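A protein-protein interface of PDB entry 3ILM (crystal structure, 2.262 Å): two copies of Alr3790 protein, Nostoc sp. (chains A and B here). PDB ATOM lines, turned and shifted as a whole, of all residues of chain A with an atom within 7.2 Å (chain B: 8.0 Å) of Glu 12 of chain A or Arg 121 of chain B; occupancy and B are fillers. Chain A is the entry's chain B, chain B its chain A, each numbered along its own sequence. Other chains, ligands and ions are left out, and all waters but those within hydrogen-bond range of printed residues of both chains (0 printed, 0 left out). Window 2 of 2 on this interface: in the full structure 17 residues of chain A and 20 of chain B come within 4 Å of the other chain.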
ATOM      1  N   HIS A   5      15.409  -8.964  -5.952  1.00  0.00           N
ATOM      2  CA  HIS A   5      14.622  -8.269  -6.974  1.00  0.00           C
ATOM      3  C   HIS A   5      14.278  -6.857  -6.530  1.00  0.00           C
ATOM      4  O   HIS A   5      14.294  -5.918  -7.328  1.00  0.00           O
ATOM      5  CB  HIS A   5      13.328  -9.035  -7.294  1.00  0.00           C
ATOM      6  CG  HIS A   5      13.523 -10.187  -8.232  1.00  0.00           C
ATOM      7  ND1 HIS A   5      13.603 -11.496  -7.806  1.00  0.00           N
ATOM      8  CD2 HIS A   5      13.691 -10.220  -9.575  1.00  0.00           C
ATOM      9  CE1 HIS A   5      13.813 -12.285  -8.845  1.00  0.00           C
ATOM     10  NE2 HIS A   5      13.871 -11.535  -9.932  1.00  0.00           N
ATOM     11  N   VAL A   6      13.972  -6.698  -5.249  1.00  0.00           N
ATOM     12  CA  VAL A   6      13.633  -5.382  -4.751  1.00  0.00           C
ATOM     13  C   VAL A   6      14.815  -4.444  -4.865  1.00  0.00           C
ATOM     14  O   VAL A   6      14.655  -3.306  -5.301  1.00  0.00           O
ATOM     15  CB  VAL A   6      13.156  -5.433  -3.295  1.00  0.00           C
ATOM     16  CG1 VAL A   6      12.859  -4.019  -2.796  1.00  0.00           C
ATOM     17  CG2 VAL A   6      11.904  -6.291  -3.198  1.00  0.00           C
ATOM     18  N   LEU A   7      16.001  -4.915  -4.486  1.00  0.00           N
ATOM     19  CA  LEU A   7      17.204  -4.086  -4.566  1.00  0.00           C
ATOM     20  C   LEU A   7      17.533  -3.763  -6.020  1.00  0.00           C
ATOM     21  O   LEU A   7      17.932  -2.653  -6.332  1.00  0.00           O
ATOM     22  CB  LEU A   7      18.409  -4.789  -3.923  1.00  0.00           C
ATOM     23  CG  LEU A   7      19.756  -4.054  -4.064  1.00  0.00           C
ATOM     24  CD1 LEU A   7      19.692  -2.724  -3.364  1.00  0.00           C
ATOM     25  CD2 LEU A   7      20.874  -4.899  -3.481  1.00  0.00           C
ATOM     26  N   LYS A   8      17.381  -4.736  -6.910  1.00  0.00           N
ATOM     27  CA  LYS A   8      17.670  -4.497  -8.314  1.00  0.00           C
ATOM     28  C   LYS A   8      16.785  -3.358  -8.826  1.00  0.00           C
ATOM     29  O   LYS A   8      17.202  -2.564  -9.669  1.00  0.00           O
ATOM     30  CB  LYS A   8      17.446  -5.775  -9.133  1.00  0.00           C
ATOM     31  CG  LYS A   8      17.749  -5.625 -10.617  1.00  0.00           C
ATOM     32  CD  LYS A   8      17.849  -6.982 -11.295  1.00  0.00           C
ATOM     33  CE  LYS A   8      17.901  -6.864 -12.811  1.00  0.00           C
ATOM     34  NZ  LYS A   8      16.585  -6.433 -13.368  1.00  0.00           N
ATOM     35  N   SER A   9      15.569  -3.269  -8.296  1.00  0.00           N
ATOM     36  CA  SER A   9      14.647  -2.208  -8.696  1.00  0.00           C
ATOM     37  C   SER A   9      14.987  -0.867  -8.043  1.00  0.00           C
ATOM     38  O   SER A   9      14.803   0.188  -8.653  1.00  0.00           O
ATOM     39  CB  SER A   9      13.213  -2.606  -8.365  1.00  0.00           C
ATOM     40  OG  SER A   9      12.850  -3.748  -9.115  1.00  0.00           O
ATOM     41  N   ARG A  10      15.474  -0.897  -6.806  1.00  0.00           N
ATOM     42  CA  ARG A  10      15.854   0.338  -6.131  1.00  0.00           C
ATOM     43  C   ARG A  10      16.990   0.983  -6.928  1.00  0.00           C
ATOM     44  O   ARG A  10      17.046   2.199  -7.054  1.00  0.00           O
ATOM     45  CB  ARG A  10      16.356   0.068  -4.703  1.00  0.00           C
ATOM     46  CG  ARG A  10      15.327  -0.457  -3.695  1.00  0.00           C
ATOM     47  CD  ARG A  10      14.318   0.592  -3.298  1.00  0.00           C
ATOM     48  NE  ARG A  10      14.920   1.729  -2.602  1.00  0.00           N
ATOM     49  CZ  ARG A  10      15.184   1.783  -1.296  1.00  0.00           C
ATOM     50  NH1 ARG A  10      14.908   0.759  -0.499  1.00  0.00           N
ATOM     51  NH2 ARG A  10      15.717   2.878  -0.781  1.00  0.00           N
ATOM     52  N   LEU A  11      17.896   0.159  -7.456  1.00  0.00           N
ATOM     53  CA  LEU A  11      19.046   0.652  -8.228  1.00  0.00           C
ATOM     54  C   LEU A  11      18.713   1.058  -9.662  1.00  0.00           C
ATOM     55  O   LEU A  11      19.347   1.951 -10.222  1.00  0.00           O
ATOM     56  CB  LEU A  11      20.164  -0.401  -8.271  1.00  0.00           C
ATOM     57  CG  LEU A  11      21.049  -0.550  -7.032  1.00  0.00           C
ATOM     58  CD1 LEU A  11      21.840  -1.844  -7.121  1.00  0.00           C
ATOM     59  CD2 LEU A  11      21.979   0.656  -6.919  1.00  0.00           C
ATOM     60  N   GLU A  12      17.736   0.388 -10.258  1.00  0.00           N
ATOM     61  CA  GLU A  12      17.339   0.693 -11.623  1.00  0.00           C
ATOM     62  C   GLU A  12      16.337   1.832 -11.676  1.00  0.00           C
ATOM     63  O   GLU A  12      16.318   2.604 -12.636  1.00  0.00           O
ATOM     64  CB  GLU A  12      16.678  -0.521 -12.272  1.00  0.00           C
ATOM     65  CG  GLU A  12      17.614  -1.612 -12.712  1.00  0.00           C
ATOM     66  CD  GLU A  12      16.866  -2.842 -13.179  1.00  0.00           C
ATOM     67  OE1 GLU A  12      17.475  -3.676 -13.879  1.00  0.00           O
ATOM     68  OE2 GLU A  12      15.670  -2.983 -12.841  1.00  0.00           O
ATOM     69  N   TRP A  13      15.524   1.949 -10.631  1.00  0.00           N
ATOM     70  CA  TRP A  13      14.458   2.938 -10.613  1.00  0.00           C
ATOM     71  C   TRP A  13      14.223   3.789  -9.390  1.00  0.00           C
ATOM     72  O   TRP A  13      13.489   4.778  -9.458  1.00  0.00           O
ATOM     73  CB  TRP A  13      13.143   2.231 -10.849  1.00  0.00           C
ATOM     74  CG  TRP A  13      13.131   1.363 -12.021  1.00  0.00           C
ATOM     75  CD1 TRP A  13      13.400   0.032 -12.066  1.00  0.00           C
ATOM     76  CD2 TRP A  13      12.811   1.765 -13.349  1.00  0.00           C
ATOM     77  NE1 TRP A  13      13.263  -0.429 -13.357  1.00  0.00           N
ATOM     78  CE2 TRP A  13      12.904   0.614 -14.158  1.00  0.00           C
ATOM     79  CE3 TRP A  13      12.455   2.984 -13.927  1.00  0.00           C
ATOM     80  CZ2 TRP A  13      12.647   0.658 -15.529  1.00  0.00           C
ATOM     81  CZ3 TRP A  13      12.201   3.023 -15.285  1.00  0.00           C
ATOM     82  CH2 TRP A  13      12.298   1.867 -16.073  1.00  0.00           C
ATOM     83  N   GLY A  14      14.807   3.425  -8.264  1.00  0.00           N
ATOM     84  CA  GLY A  14      14.487   4.181  -7.072  1.00  0.00           C
ATOM     85  C   GLY A  14      15.257   5.405  -6.668  1.00  0.00           C
ATOM     86  O   GLY A  14      15.705   6.213  -7.498  1.00  0.00           O
ATOM     87  N   PHE A  18      19.436   4.196   0.116  1.00  0.00           N
ATOM     88  CA  PHE A  18      19.808   2.936   0.741  1.00  0.00           C
ATOM     89  C   PHE A  18      21.295   2.603   0.758  1.00  0.00           C
ATOM     90  O   PHE A  18      22.082   3.150  -0.005  1.00  0.00           O
ATOM     91  CB  PHE A  18      19.038   1.781   0.071  1.00  0.00           C
ATOM     92  CG  PHE A  18      19.327   1.634  -1.398  1.00  0.00           C
ATOM     93  CD1 PHE A  18      20.316   0.779  -1.849  1.00  0.00           C
ATOM     94  CD2 PHE A  18      18.614   2.372  -2.335  1.00  0.00           C
ATOM     95  CE1 PHE A  18      20.608   0.681  -3.217  1.00  0.00           C
ATOM     96  CE2 PHE A  18      18.899   2.283  -3.696  1.00  0.00           C
ATOM     97  CZ  PHE A  18      19.888   1.432  -4.138  1.00  0.00           C
ATOM     98  N   ILE A  97      19.993 -13.189 -11.201  1.00  0.00           N
ATOM     99  CA  ILE A  97      19.012 -12.322 -11.856  1.00  0.00           C
ATOM    100  C   ILE A  97      19.589 -11.124 -12.605  1.00  0.00           C
ATOM    101  O   ILE A  97      18.887 -10.152 -12.860  1.00  0.00           O
ATOM    102  CB  ILE A  97      17.951 -11.803 -10.862  1.00  0.00           C
ATOM    103  CG1 ILE A  97      18.503 -10.637 -10.042  1.00  0.00           C
ATOM    104  CG2 ILE A  97      17.523 -12.928  -9.930  1.00  0.00           C
ATOM    105  CD1 ILE A  97      17.443  -9.914  -9.226  1.00  0.00           C
ATOM    106  N   GLY A  98      20.867 -11.193 -12.954  1.00  0.00           N
ATOM    107  CA  GLY A  98      21.488 -10.107 -13.696  1.00  0.00           C
ATOM    108  C   GLY A  98      22.147  -9.038 -12.850  1.00  0.00           C
ATOM    109  O   GLY A  98      22.535  -7.990 -13.368  1.00  0.00           O
ATOM    110  N   VAL B 119      22.032  -3.090 -16.552  1.00  0.00           N
ATOM    111  CA  VAL B 119      23.148  -2.742 -15.676  1.00  0.00           C
ATOM    112  C   VAL B 119      23.855  -1.458 -16.152  1.00  0.00           C
ATOM    113  O   VAL B 119      24.775  -0.953 -15.503  1.00  0.00           O
ATOM    114  CB  VAL B 119      24.125  -3.958 -15.533  1.00  0.00           C
ATOM    115  CG1 VAL B 119      23.885  -4.947 -16.666  1.00  0.00           C
ATOM    116  CG2 VAL B 119      25.578  -3.502 -15.504  1.00  0.00           C
ATOM    117  N   SER B 120      23.406  -0.937 -17.290  1.00  0.00           N
ATOM    118  CA  SER B 120      23.926   0.319 -17.818  1.00  0.00           C
ATOM    119  C   SER B 120      22.832   1.293 -17.377  1.00  0.00           C
ATOM    120  O   SER B 120      23.033   2.510 -17.295  1.00  0.00           O
ATOM    121  CB  SER B 120      24.033   0.280 -19.349  1.00  0.00           C
ATOM    122  OG  SER B 120      22.760   0.218 -19.972  1.00  0.00           O
ATOM    123  N   ARG B 121      21.671   0.709 -17.082  1.00  0.00           N
ATOM    124  CA  ARG B 121      20.491   1.429 -16.610  1.00  0.00           C
ATOM    125  C   ARG B 121      20.667   1.758 -15.130  1.00  0.00           C
ATOM    126  O   ARG B 121      20.183   2.786 -14.662  1.00  0.00           O
ATOM    127  CB  ARG B 121      19.242   0.564 -16.798  1.00  0.00           C
ATOM    128  CG  ARG B 121      18.018   1.041 -16.023  1.00  0.00           C
ATOM    129  CD  ARG B 121      16.924  -0.010 -16.060  1.00  0.00           C
ATOM    130  NE  ARG B 121      16.324  -0.145 -17.386  1.00  0.00           N
ATOM    131  CZ  ARG B 121      15.708  -1.243 -17.815  1.00  0.00           C
ATOM    132  NH1 ARG B 121      15.619  -2.308 -17.025  1.00  0.00           N
ATOM    133  NH2 ARG B 121      15.176  -1.278 -19.031  1.00  0.00           N
ATOM    134  N   MET B 122      21.337   0.872 -14.394  1.00  0.00           N
ATOM    135  CA  MET B 122      21.587   1.115 -12.977  1.00  0.00           C
ATOM    136  C   MET B 122      22.576   2.263 -12.927  1.00  0.00           C
ATOM    137  O   MET B 122      22.413   3.207 -12.157  1.00  0.00           O
ATOM    138  CB  MET B 122      22.247  -0.082 -12.297  1.00  0.00           C
ATOM    139  CG  MET B 122      21.519  -1.394 -12.417  1.00  0.00           C
ATOM    140  SD  MET B 122      22.309  -2.702 -11.222  1.00  0.00           S
ATOM    141  CE  MET B 122      23.853  -1.696 -10.568  1.00  0.00           C
ATOM    142  N   GLN B 123      23.606   2.154 -13.764  1.00  0.00           N
ATOM    143  CA  GLN B 123      24.669   3.148 -13.857  1.00  0.00           C
ATOM    144  C   GLN B 123      24.209   4.521 -14.338  1.00  0.00           C
ATOM    145  O   GLN B 123      24.636   5.534 -13.790  1.00  0.00           O
ATOM    146  CB  GLN B 123      25.791   2.637 -14.768  1.00  0.00           C
ATOM    147  CG  GLN B 123      26.971   2.002 -14.033  1.00  0.00           C
ATOM    148  CD  GLN B 123      28.031   1.449 -14.983  1.00  0.00           C
ATOM    149  OE1 GLN B 123      29.175   1.215 -14.587  1.00  0.00           O
ATOM    150  NE2 GLN B 123      27.648   1.227 -16.241  1.00  0.00           N
ATOM    151  N   ASN B 124      23.355   4.572 -15.358  1.00  0.00           N
ATOM    152  CA  ASN B 124      22.900   5.870 -15.838  1.00  0.00           C
ATOM    153  C   ASN B 124      21.921   6.493 -14.849  1.00  0.00           C
ATOM    154  O   ASN B 124      22.062   7.652 -14.466  1.00  0.00           O
ATOM    155  CB  ASN B 124      22.241   5.762 -17.214  1.00  0.00           C
ATOM    156  CG  ASN B 124      22.146   7.112 -17.907  1.00  0.00           C
ATOM    157  OD1 ASN B 124      23.020   7.483 -18.691  1.00  0.00           O
ATOM    158  ND2 ASN B 124      21.095   7.866 -17.597  1.00  0.00           N
ATOM    159  N   HIS B 125      20.922   5.722 -14.441  1.00  0.00           N
ATOM    160  CA  HIS B 125      19.949   6.217 -13.478  1.00  0.00           C
ATOM    161  C   HIS B 125      20.711   6.813 -12.296  1.00  0.00           C
ATOM    162  O   HIS B 125      20.343   7.870 -11.787  1.00  0.00           O
ATOM    163  CB  HIS B 125      19.048   5.069 -12.999  1.00  0.00           C
ATOM    164  CG  HIS B 125      18.109   5.454 -11.896  1.00  0.00           C
ATOM    165  ND1 HIS B 125      18.246   4.992 -10.604  1.00  0.00           N
ATOM    166  CD2 HIS B 125      17.027   6.267 -11.892  1.00  0.00           C
ATOM    167  CE1 HIS B 125      17.288   5.502  -9.853  1.00  0.00           C
ATOM    168  NE2 HIS B 125      16.534   6.280 -10.609  1.00  0.00           N
ATOM    169  N   LEU B 126      21.781   6.121 -11.902  1.00  0.00           N
ATOM    170  CA  LEU B 126      22.670   6.471 -10.786  1.00  0.00           C
ATOM    171  C   LEU B 126      22.725   7.918 -10.289  1.00  0.00           C
ATOM    172  O   LEU B 126      23.573   8.178  -9.410  1.00  0.00           O
ATOM    173  CB  LEU B 126      24.086   6.006 -11.112  1.00  0.00           C
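Of the 8 printed residues of chain B, 3 touch a printed residue of chain A. Hydrophobic or aromatic side chains of chain B that line the printed part of chain A: Met 122 and His 125. Among the printed residues, Asp or Glu carboxylates within 4 Å of a Lys or Arg side-chain nitrogen of the other chain: Glu 12 of chain A with Arg 121 of chain B (3.9 Å).
Among the printed residues, merely in contact across the chains: Glu 12 of chain A with His 125 of chain B (3.4 Å), Trp 13 of chain A with His 125 of chain B (3.5 Å), Leu 11 of chain A with Met 122 of chain B (3.6 Å) and Glu 12 of chain A with Met 122 of chain B (3.9 Å).
No position is printed for both chains.
Leu 7 of chain A touches none of the printed residues of chain B. Printed residues of chain B within 4 Å of Leu 11 of chain A: Met 122 (3.6 Å) and His 125 (3.3 Å). Glu 12 of chain A touches just these residues of chain B: Arg 121 (3.8 Å), Met 122 (3.9 Å) and His 125 (3.4 Å). Printed residues of chain B within 4 Å of Trp 13 of chain A: His 125. Of the printed residues of chain B, Gly 14 of chain A touches His 125 (2.9 Å). Phe 18 of chain A touches none of the printed residues of chain B. Arg 121 of chain B touches one residue of chain A. Printed residues of chain A within 4 Å of Met 122 of chain B: Leu 11 (3.6 Å) and Glu 12 (3.9 Å). Of the printed residues of chain A, His 125 of chain B touches Leu 11, Glu 12, Trp 13 and Gly 14. The nearest printed residue of chain B that does not touch Trp 13 of chain A is Arg 121 of chain B (4.2 Å).
O of Ser 9 of chain A lies within hydrogen-bond range of N of Gly 14 of chain A. The side-chain amino group (NZ) of Lys 8 of chain A lies within salt-bridge range of the side-chain carboxylate (OE1) of Glu 12 of chain A.
NE2 of His 125 of chain B lies close to O of Gly 14 of chain A (3.2 Å). The guanidinium group (NH1) of Arg 121 of chain B is in salt-bridge range of the side-chain carboxylate (OE1) of Glu 12 of chain A. The backbone carbonyl oxygen (O) of Leu 11 of chain A sits at hydrogen-bond distance from a ring nitrogen (ND1) of His 125 of chain B, 3.3 Å away.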
